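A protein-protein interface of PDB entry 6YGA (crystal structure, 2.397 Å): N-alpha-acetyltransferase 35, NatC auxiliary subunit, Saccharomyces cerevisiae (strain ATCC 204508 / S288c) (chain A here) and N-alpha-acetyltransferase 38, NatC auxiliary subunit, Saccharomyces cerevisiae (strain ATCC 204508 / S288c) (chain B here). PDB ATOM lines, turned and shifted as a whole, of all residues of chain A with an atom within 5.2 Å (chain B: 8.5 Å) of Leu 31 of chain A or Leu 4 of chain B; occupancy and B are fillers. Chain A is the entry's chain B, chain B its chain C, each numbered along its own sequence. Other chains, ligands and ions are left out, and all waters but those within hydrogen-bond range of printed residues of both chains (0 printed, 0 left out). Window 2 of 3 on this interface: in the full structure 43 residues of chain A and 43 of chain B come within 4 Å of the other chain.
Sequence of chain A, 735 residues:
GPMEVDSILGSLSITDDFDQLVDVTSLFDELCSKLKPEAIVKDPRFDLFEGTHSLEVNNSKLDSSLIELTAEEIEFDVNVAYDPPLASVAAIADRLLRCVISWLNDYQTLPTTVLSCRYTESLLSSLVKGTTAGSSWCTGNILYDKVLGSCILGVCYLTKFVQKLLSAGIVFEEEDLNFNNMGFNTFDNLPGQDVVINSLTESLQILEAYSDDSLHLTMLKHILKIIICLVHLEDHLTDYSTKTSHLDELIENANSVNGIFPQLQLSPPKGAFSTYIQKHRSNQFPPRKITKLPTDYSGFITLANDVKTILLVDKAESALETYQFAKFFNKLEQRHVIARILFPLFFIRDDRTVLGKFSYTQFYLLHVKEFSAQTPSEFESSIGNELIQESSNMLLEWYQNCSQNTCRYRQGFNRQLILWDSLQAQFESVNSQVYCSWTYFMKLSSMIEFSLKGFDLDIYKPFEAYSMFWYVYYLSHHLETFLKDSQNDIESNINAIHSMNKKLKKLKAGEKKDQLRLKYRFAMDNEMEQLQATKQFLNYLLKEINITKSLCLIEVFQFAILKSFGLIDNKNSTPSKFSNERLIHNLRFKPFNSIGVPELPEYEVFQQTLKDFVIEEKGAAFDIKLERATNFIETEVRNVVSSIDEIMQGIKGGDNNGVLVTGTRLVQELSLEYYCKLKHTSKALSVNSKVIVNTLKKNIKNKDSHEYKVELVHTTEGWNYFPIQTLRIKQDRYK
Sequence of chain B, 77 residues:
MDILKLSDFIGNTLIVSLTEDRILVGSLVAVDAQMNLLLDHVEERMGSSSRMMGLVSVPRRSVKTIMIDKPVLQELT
Of chain B, only Leu 4, Lys 5 and Leu 6 come within 4 Å of Leu 31 of chain A. Of the printed residues of chain B, Cys 32 of chain A touches Leu 6, Val 31, Asp 32, Ala 33 and Met 35. Of chain A, only Leu 27 and Leu 31 come within 4 Å of Leu 4 of chain B. Of the printed residues of chain A, Lys 5 of chain B touches Leu 31 (3.7 Å). Printed residues of chain A within 4 Å of Phe 9 of chain B: Phe 28. Of the printed residues of chain A, Val 31 of chain B touches Cys 32 (3.7 Å). Leu 76 of chain B touches none of the printed residues of chain A. The nearest printed residue of chain A that does not touch Leu 4 of chain B is Lys 34 of chain A (6.5 Å). The nearest printed residue of chain B that does not touch Leu 35 of chain A is Ala 33 of chain B (4.1 Å).
Leu 27 of chain A touches Leu 4 of chain B. Phe 28 of chain A touches Phe 9 of chain B (CE1 to CD2, 3.3 Å). Leu 4 of chain B touches Leu 31 of chain A. Lys 5 of chain B touches Leu 31 of chain A. Leu 6 of chain B touches Leu 31 of chain A. Leu 6 of chain B touches Cys 32 of chain A. Cys 32 of chain A touches Val 31 of chain B. CG of Met 35 of chain B touches SG of Cys 32 of chain A (3.9 Å). Leu 35 of chain A touches Leu 6 of chain B. Leu 35 of chain A touches Asp 32 of chain B.
Of the 17 printed residues of chain B, 8 touch a printed residue of chain A. Hydrophobic or aromatic side chains of chain B within 4 Å of the printed part of chain A: Leu 4, Leu 6, Phe 9, Val 31 and Met 35. Printed residues of chain A that touch a printed residue of chain B: Leu 27, Phe 28, Leu 31, Cys 32 and Leu 35. Hydrophobic or aromatic side chains of chain A within 4 Å of the printed part of chain B: Leu 27, Phe 28, Leu 31 and Leu 35. Among the printed residues, no Asp or Glu carboxylate lies within 4 Å of a Lys or Arg side-chain nitrogen of the other chain.
O of Cys 32 of chain A sits close to O of Ala 33 of chain B. The side-chain sulfur of Cys 32 of chain A lies within hydrogen-bond range of the backbone carbonyl oxygen of Asp 32 of chain B (3.7 Å).
The backbone carbonyl oxygen (O) of Phe 28 of chain A sits at hydrogen-bond distance from the side-chain sulfur (SG) of Cys 32 of chain A (3.2 Å). The side-chain carboxylate (OD2) of Asp 8 of chain B lies within hydrogen-bond range of the backbone NH (N) of Lys 5 of chain B, 2.8 Å away. The side-chain carboxylate (OD1) of Asp 32 of chain B sits at hydrogen-bond distance from the backbone NH (N) of Met 35 of chain B (3.2 Å).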
ATOM      1  N   LEU A  27       7.041 -16.118  12.604  1.00  0.00           N
ATOM      2  CA  LEU A  27       6.360 -16.227  11.316  1.00  0.00           C
ATOM      3  C   LEU A  27       5.845 -14.872  10.846  1.00  0.00           C
ATOM      4  O   LEU A  27       5.850 -14.581   9.643  1.00  0.00           O
ATOM      5  CB  LEU A  27       5.210 -17.233  11.404  1.00  0.00           C
ATOM      6  CG  LEU A  27       4.328 -17.351  10.154  1.00  0.00           C
ATOM      7  CD1 LEU A  27       5.152 -17.788   8.950  1.00  0.00           C
ATOM      8  CD2 LEU A  27       3.150 -18.295  10.373  1.00  0.00           C
ATOM      9  N   PHE A  28       5.404 -14.026  11.779  1.00  0.00           N
ATOM     10  CA  PHE A  28       4.869 -12.723  11.399  1.00  0.00           C
ATOM     11  C   PHE A  28       5.944 -11.830  10.793  1.00  0.00           C
ATOM     12  O   PHE A  28       5.668 -11.067   9.859  1.00  0.00           O
ATOM     13  CB  PHE A  28       4.235 -12.044  12.612  1.00  0.00           C
ATOM     14  CG  PHE A  28       2.734 -12.070  12.602  1.00  0.00           C
ATOM     15  CD1 PHE A  28       2.051 -13.261  12.403  1.00  0.00           C
ATOM     16  CD2 PHE A  28       2.002 -10.909  12.794  1.00  0.00           C
ATOM     17  CE1 PHE A  28       0.667 -13.295  12.390  1.00  0.00           C
ATOM     18  CE2 PHE A  28       0.614 -10.937  12.785  1.00  0.00           C
ATOM     19  CZ  PHE A  28      -0.055 -12.134  12.582  1.00  0.00           C
ATOM     20  N   ASP A  29       7.171 -11.901  11.311  1.00  0.00           N
ATOM     21  CA  ASP A  29       8.216 -11.007  10.826  1.00  0.00           C
ATOM     22  C   ASP A  29       8.730 -11.442   9.457  1.00  0.00           C
ATOM     23  O   ASP A  29       9.031 -10.594   8.608  1.00  0.00           O
ATOM     24  CB  ASP A  29       9.360 -10.935  11.839  1.00  0.00           C
ATOM     25  CG  ASP A  29      10.131  -9.626  11.761  1.00  0.00           C
ATOM     26  OD1 ASP A  29      10.013  -8.918  10.740  1.00  0.00           O
ATOM     27  OD2 ASP A  29      10.860  -9.308  12.726  1.00  0.00           O
ATOM     28  N   GLU A  30       8.845 -12.755   9.227  1.00  0.00           N
ATOM     29  CA  GLU A  30       9.238 -13.250   7.910  1.00  0.00           C
ATOM     30  C   GLU A  30       8.272 -12.769   6.835  1.00  0.00           C
ATOM     31  O   GLU A  30       8.688 -12.204   5.817  1.00  0.00           O
ATOM     32  CB  GLU A  30       9.291 -14.778   7.911  1.00  0.00           C
ATOM     33  CG  GLU A  30      10.101 -15.417   9.018  1.00  0.00           C
ATOM     34  CD  GLU A  30      10.007 -16.929   8.969  1.00  0.00           C
ATOM     35  OE1 GLU A  30       9.643 -17.456   7.898  1.00  0.00           O
ATOM     36  OE2 GLU A  30      10.280 -17.590   9.994  1.00  0.00           O
ATOM     37  N   LEU A  31       6.973 -12.993   7.047  1.00  0.00           N
ATOM     38  CA  LEU A  31       5.979 -12.617   6.048  1.00  0.00           C
ATOM     39  C   LEU A  31       5.954 -11.110   5.823  1.00  0.00           C
ATOM     40  O   LEU A  31       5.837 -10.651   4.682  1.00  0.00           O
ATOM     41  CB  LEU A  31       4.596 -13.112   6.469  1.00  0.00           C
ATOM     42  CG  LEU A  31       4.384 -14.627   6.494  1.00  0.00           C
ATOM     43  CD1 LEU A  31       2.972 -14.982   6.944  1.00  0.00           C
ATOM     44  CD2 LEU A  31       4.677 -15.219   5.125  1.00  0.00           C
ATOM     45  N   CYS A  32       6.053 -10.326   6.902  1.00  0.00           N
ATOM     46  CA  CYS A  32       6.017  -8.872   6.760  1.00  0.00           C
ATOM     47  C   CYS A  32       7.214  -8.355   5.975  1.00  0.00           C
ATOM     48  O   CYS A  32       7.110  -7.331   5.290  1.00  0.00           O
ATOM     49  CB  CYS A  32       5.955  -8.202   8.135  1.00  0.00           C
ATOM     50  SG  CYS A  32       4.353  -8.324   8.966  1.00  0.00           S
ATOM     51  N   SER A  33       8.352  -9.047   6.055  1.00  0.00           N
ATOM     52  CA  SER A  33       9.521  -8.636   5.286  1.00  0.00           C
ATOM     53  C   SER A  33       9.296  -8.794   3.788  1.00  0.00           C
ATOM     54  O   SER A  33       9.812  -7.998   2.995  1.00  0.00           O
ATOM     55  CB  SER A  33      10.745  -9.434   5.731  1.00  0.00           C
ATOM     56  OG  SER A  33      11.240  -8.965   6.973  1.00  0.00           O
ATOM     57  N   LYS A  34       8.527  -9.805   3.378  1.00  0.00           N
ATOM     58  CA  LYS A  34       8.260 -10.008   1.960  1.00  0.00           C
ATOM     59  C   LYS A  34       7.308  -8.962   1.398  1.00  0.00           C
ATOM     60  O   LYS A  34       7.276  -8.768   0.178  1.00  0.00           O
ATOM     61  CB  LYS A  34       7.693 -11.410   1.727  1.00  0.00           C
ATOM     62  CG  LYS A  34       8.588 -12.526   2.243  1.00  0.00           C
ATOM     63  CD  LYS A  34       7.930 -13.889   2.103  1.00  0.00           C
ATOM     64  CE  LYS A  34       8.875 -14.998   2.541  1.00  0.00           C
ATOM     65  NZ  LYS A  34       8.244 -16.341   2.437  1.00  0.00           N
ATOM     66  N   LEU A  35       6.543  -8.285   2.249  1.00  0.00           N
ATOM     67  CA  LEU A  35       5.606  -7.275   1.777  1.00  0.00           C
ATOM     68  C   LEU A  35       6.341  -6.058   1.229  1.00  0.00           C
ATOM     69  O   LEU A  35       7.375  -5.644   1.762  1.00  0.00           O
ATOM     70  CB  LEU A  35       4.682  -6.836   2.913  1.00  0.00           C
ATOM     71  CG  LEU A  35       3.866  -7.895   3.652  1.00  0.00           C
ATOM     72  CD1 LEU A  35       3.229  -7.280   4.888  1.00  0.00           C
ATOM     73  CD2 LEU A  35       2.805  -8.493   2.743  1.00  0.00           C
ATOM     74  N   ILE B   3       1.591 -24.162   3.404  1.00  0.00           N
ATOM     75  CA  ILE B   3       2.218 -22.848   3.334  1.00  0.00           C
ATOM     76  C   ILE B   3       1.236 -21.804   3.865  1.00  0.00           C
ATOM     77  O   ILE B   3       0.020 -22.000   3.805  1.00  0.00           O
ATOM     78  CB  ILE B   3       2.679 -22.517   1.897  1.00  0.00           C
ATOM     79  CG1 ILE B   3       2.941 -23.803   1.097  1.00  0.00           C
ATOM     80  CG2 ILE B   3       3.922 -21.634   1.937  1.00  0.00           C
ATOM     81  CD1 ILE B   3       3.313 -23.590  -0.382  1.00  0.00           C
ATOM     82  N   LEU B   4       1.756 -20.693   4.383  1.00  0.00           N
ATOM     83  CA  LEU B   4       0.924 -19.719   5.074  1.00  0.00           C
ATOM     84  C   LEU B   4       1.142 -18.312   4.535  1.00  0.00           C
ATOM     85  O   LEU B   4       2.160 -18.001   3.911  1.00  0.00           O
ATOM     86  CB  LEU B   4       1.179 -19.732   6.587  1.00  0.00           C
ATOM     87  CG  LEU B   4       0.264 -20.679   7.364  1.00  0.00           C
ATOM     88  CD1 LEU B   4       0.376 -20.428   8.857  1.00  0.00           C
ATOM     89  CD2 LEU B   4      -1.177 -20.530   6.892  1.00  0.00           C
ATOM     90  N   LYS B   5       0.149 -17.464   4.796  1.00  0.00           N
ATOM     91  CA  LYS B   5       0.180 -16.055   4.445  1.00  0.00           C
ATOM     92  C   LYS B   5      -0.448 -15.262   5.581  1.00  0.00           C
ATOM     93  O   LYS B   5      -1.219 -15.795   6.382  1.00  0.00           O
ATOM     94  CB  LYS B   5      -0.569 -15.782   3.135  1.00  0.00           C
ATOM     95  CG  LYS B   5       0.159 -16.231   1.881  1.00  0.00           C
ATOM     96  CD  LYS B   5       1.384 -15.367   1.623  1.00  0.00           C
ATOM     97  CE  LYS B   5       1.941 -15.590   0.225  1.00  0.00           C
ATOM     98  NZ  LYS B   5       1.003 -15.121  -0.832  1.00  0.00           N
ATOM     99  N   LEU B   6      -0.112 -13.972   5.643  1.00  0.00           N
ATOM    100  CA  LEU B   6      -0.740 -13.094   6.626  1.00  0.00           C
ATOM    101  C   LEU B   6      -2.241 -12.972   6.392  1.00  0.00           C
ATOM    102  O   LEU B   6      -3.004 -12.782   7.346  1.00  0.00           O
ATOM    103  CB  LEU B   6      -0.084 -11.717   6.590  1.00  0.00           C
ATOM    104  CG  LEU B   6       1.361 -11.633   7.071  1.00  0.00           C
ATOM    105  CD1 LEU B   6       1.974 -10.319   6.631  1.00  0.00           C
ATOM    106  CD2 LEU B   6       1.420 -11.772   8.585  1.00  0.00           C
ATOM    107  N   SER B   7      -2.681 -13.084   5.134  1.00  0.00           N
ATOM    108  CA  SER B   7      -4.103 -13.010   4.819  1.00  0.00           C
ATOM    109  C   SER B   7      -4.905 -14.068   5.563  1.00  0.00           C
ATOM    110  O   SER B   7      -6.076 -13.845   5.887  1.00  0.00           O
ATOM    111  CB  SER B   7      -4.312 -13.161   3.312  1.00  0.00           C
ATOM    112  OG  SER B   7      -5.680 -13.042   2.968  1.00  0.00           O
ATOM    113  N   ASP B   8      -4.296 -15.222   5.844  1.00  0.00           N
ATOM    114  CA  ASP B   8      -4.999 -16.266   6.583  1.00  0.00           C
ATOM    115  C   ASP B   8      -5.276 -15.843   8.019  1.00  0.00           C
ATOM    116  O   ASP B   8      -6.222 -16.338   8.642  1.00  0.00           O
ATOM    117  CB  ASP B   8      -4.183 -17.561   6.569  1.00  0.00           C
ATOM    118  CG  ASP B   8      -3.823 -18.012   5.166  1.00  0.00           C
ATOM    119  OD1 ASP B   8      -4.745 -18.275   4.366  1.00  0.00           O
ATOM    120  OD2 ASP B   8      -2.615 -18.106   4.863  1.00  0.00           O
ATOM    121  N   PHE B   9      -4.468 -14.926   8.557  1.00  0.00           N
ATOM    122  CA  PHE B   9      -4.532 -14.604   9.978  1.00  0.00           C
ATOM    123  C   PHE B   9      -5.596 -13.565  10.309  1.00  0.00           C
ATOM    124  O   PHE B   9      -6.160 -13.601  11.410  1.00  0.00           O
ATOM    125  CB  PHE B   9      -3.169 -14.110  10.463  1.00  0.00           C
ATOM    126  CG  PHE B   9      -2.247 -15.208  10.902  1.00  0.00           C
ATOM    127  CD1 PHE B   9      -1.687 -16.076   9.980  1.00  0.00           C
ATOM    128  CD2 PHE B   9      -1.932 -15.364  12.240  1.00  0.00           C
ATOM    129  CE1 PHE B   9      -0.831 -17.086  10.390  1.00  0.00           C
ATOM    130  CE2 PHE B   9      -1.077 -16.366  12.657  1.00  0.00           C
ATOM    131  CZ  PHE B   9      -0.526 -17.229  11.732  1.00  0.00           C
ATOM    132  N   VAL B  31      -2.265  -5.426   9.055  1.00  0.00           N
ATOM    133  CA  VAL B  31      -0.831  -5.416   9.319  1.00  0.00           C
ATOM    134  C   VAL B  31      -0.144  -4.791   8.111  1.00  0.00           C
ATOM    135  O   VAL B  31      -0.581  -4.984   6.972  1.00  0.00           O
ATOM    136  CB  VAL B  31      -0.288  -6.836   9.612  1.00  0.00           C
ATOM    137  CG1 VAL B  31      -0.499  -7.763   8.420  1.00  0.00           C
ATOM    138  CG2 VAL B  31       1.185  -6.788  10.007  1.00  0.00           C
ATOM    139  N   ASP B  32       0.909  -4.013   8.359  1.00  0.00           N
ATOM    140  CA  ASP B  32       1.640  -3.335   7.298  1.00  0.00           C
ATOM    141  C   ASP B  32       3.042  -3.931   7.159  1.00  0.00           C
ATOM    142  O   ASP B  32       3.380  -4.943   7.783  1.00  0.00           O
ATOM    143  CB  ASP B  32       1.684  -1.824   7.555  1.00  0.00           C
ATOM    144  CG  ASP B  32       2.444  -1.457   8.819  1.00  0.00           C
ATOM    145  OD1 ASP B  32       2.882  -2.368   9.551  1.00  0.00           O
ATOM    146  OD2 ASP B  32       2.599  -0.243   9.078  1.00  0.00           O
ATOM    147  N   ALA B  33       3.869  -3.279   6.338  1.00  0.00           N
ATOM    148  CA  ALA B  33       5.188  -3.818   6.023  1.00  0.00           C
ATOM    149  C   ALA B  33       6.129  -3.760   7.219  1.00  0.00           C
ATOM    150  O   ALA B  33       7.046  -4.584   7.324  1.00  0.00           O
ATOM    151  CB  ALA B  33       5.790  -3.062   4.839  1.00  0.00           C
ATOM    152  N   MET B  35       5.314  -4.313  10.330  1.00  0.00           N
ATOM    153  CA  MET B  35       4.718  -5.111  11.403  1.00  0.00           C
ATOM    154  C   MET B  35       3.943  -4.267  12.416  1.00  0.00           C
ATOM    155  O   MET B  35       3.813  -4.655  13.577  1.00  0.00           O
ATOM    156  CB  MET B  35       5.786  -5.943  12.126  1.00  0.00           C
ATOM    157  CG  MET B  35       5.280  -7.297  12.613  1.00  0.00           C
ATOM    158  SD  MET B  35       6.565  -8.292  13.693  1.00  0.00           S
ATOM    159  CE  MET B  35       6.454  -7.258  15.343  1.00  0.00           C
ATOM    160  N   ILE B  68      -1.090 -17.161  19.097  1.00  0.00           N
ATOM    161  CA  ILE B  68      -2.418 -17.551  18.643  1.00  0.00           C
ATOM    162  C   ILE B  68      -2.777 -18.887  19.281  1.00  0.00           C
ATOM    163  O   ILE B  68      -1.900 -19.690  19.621  1.00  0.00           O
ATOM    164  CB  ILE B  68      -2.505 -17.632  17.098  1.00  0.00           C
ATOM    165  CG1 ILE B  68      -3.964 -17.657  16.631  1.00  0.00           C
ATOM    166  CG2 ILE B  68      -1.774 -18.857  16.576  1.00  0.00           C
ATOM    167  CD1 ILE B  68      -4.126 -17.783  15.128  1.00  0.00           C
ATOM    168  N   LEU B  73      -5.131 -21.852  15.102  1.00  0.00           N
ATOM    169  CA  LEU B  73      -4.040 -21.792  14.130  1.00  0.00           C
ATOM    170  C   LEU B  73      -4.167 -22.887  13.077  1.00  0.00           C
ATOM    171  O   LEU B  73      -4.016 -22.631  11.877  1.00  0.00           O
ATOM    172  CB  LEU B  73      -2.694 -21.895  14.850  1.00  0.00           C
ATOM    173  CG  LEU B  73      -1.457 -22.166  13.988  1.00  0.00           C
ATOM    174  CD1 LEU B  73      -1.258 -21.070  12.951  1.00  0.00           C
ATOM    175  CD2 LEU B  73      -0.217 -22.316  14.862  1.00  0.00           C
ATOM    176  N   GLN B  74      -4.433 -24.123  13.510  1.00  0.00           N
ATOM    177  CA  GLN B  74      -4.572 -25.220  12.558  1.00  0.00           C
ATOM    178  C   GLN B  74      -5.800 -25.039  11.674  1.00  0.00           C
ATOM    179  O   GLN B  74      -5.823 -25.522  10.536  1.00  0.00           O
ATOM    180  CB  GLN B  74      -4.642 -26.555  13.302  1.00  0.00           C
ATOM    181  CG  GLN B  74      -3.690 -26.667  14.491  1.00  0.00           C
ATOM    182  CD  GLN B  74      -2.229 -26.481  14.114  1.00  0.00           C
ATOM    183  OE1 GLN B  74      -1.835 -26.690  12.966  1.00  0.00           O
ATOM    184  NE2 GLN B  74      -1.417 -26.089  15.088  1.00  0.00           N
ATOM    185  N   GLU B  75      -6.818 -24.338  12.177  1.00  0.00           N
ATOM    186  CA  GLU B  75      -8.030 -24.115  11.397  1.00  0.00           C
ATOM    187  C   GLU B  75      -7.758 -23.205  10.205  1.00  0.00           C
ATOM    188  O   GLU B  75      -8.345 -23.386   9.133  1.00  0.00           O
ATOM    189  CB  GLU B  75      -9.111 -23.519  12.297  1.00  0.00           C
ATOM    190  CG  GLU B  75     -10.533 -23.929  11.963  1.00  0.00           C
ATOM    191  CD  GLU B  75     -11.518 -23.456  13.016  1.00  0.00           C
ATOM    192  OE1 GLU B  75     -11.068 -22.994  14.087  1.00  0.00           O
ATOM    193  OE2 GLU B  75     -12.740 -23.539  12.776  1.00  0.00           O
ATOM    194  N   LEU B  76      -6.864 -22.227  10.371  1.00  0.00           N
ATOM    195  CA  LEU B  76      -6.580 -21.284   9.292  1.00  0.00           C
ATOM    196  C   LEU B  76      -5.959 -21.980   8.086  1.00  0.00           C
ATOM    197  O   LEU B  76      -6.222 -21.599   6.939  1.00  0.00           O
ATOM    198  CB  LEU B  76      -5.652 -20.178   9.791  1.00  0.00           C
ATOM    199  CG  LEU B  76      -5.865 -19.668  11.215  1.00  0.00           C
ATOM    200  CD1 LEU B  76      -4.857 -18.580  11.545  1.00  0.00           C
ATOM    201  CD2 LEU B  76      -7.287 -19.169  11.404  1.00  0.00           C
ATOM    202  N   THR B  77      -5.125 -22.990   8.323  1.00  0.00           N
ATOM    203  CA  THR B  77      -4.398 -23.682   7.258  1.00  0.00           C
ATOM    204  C   THR B  77      -5.343 -24.401   6.291  1.00  0.00           C
ATOM    205  O   THR B  77      -4.920 -24.893   5.232  1.00  0.00           O
ATOM    206  CB  THR B  77      -3.403 -24.710   7.845  1.00  0.00           C
ATOM    207  OG1 THR B  77      -4.121 -25.867   8.284  1.00  0.00           O
ATOM    208  CG2 THR B  77      -2.653 -24.124   9.046  1.00  0.00           C
ATOM    209  OXT THR B  77      -6.545 -24.496   6.573  1.00  0.00           O
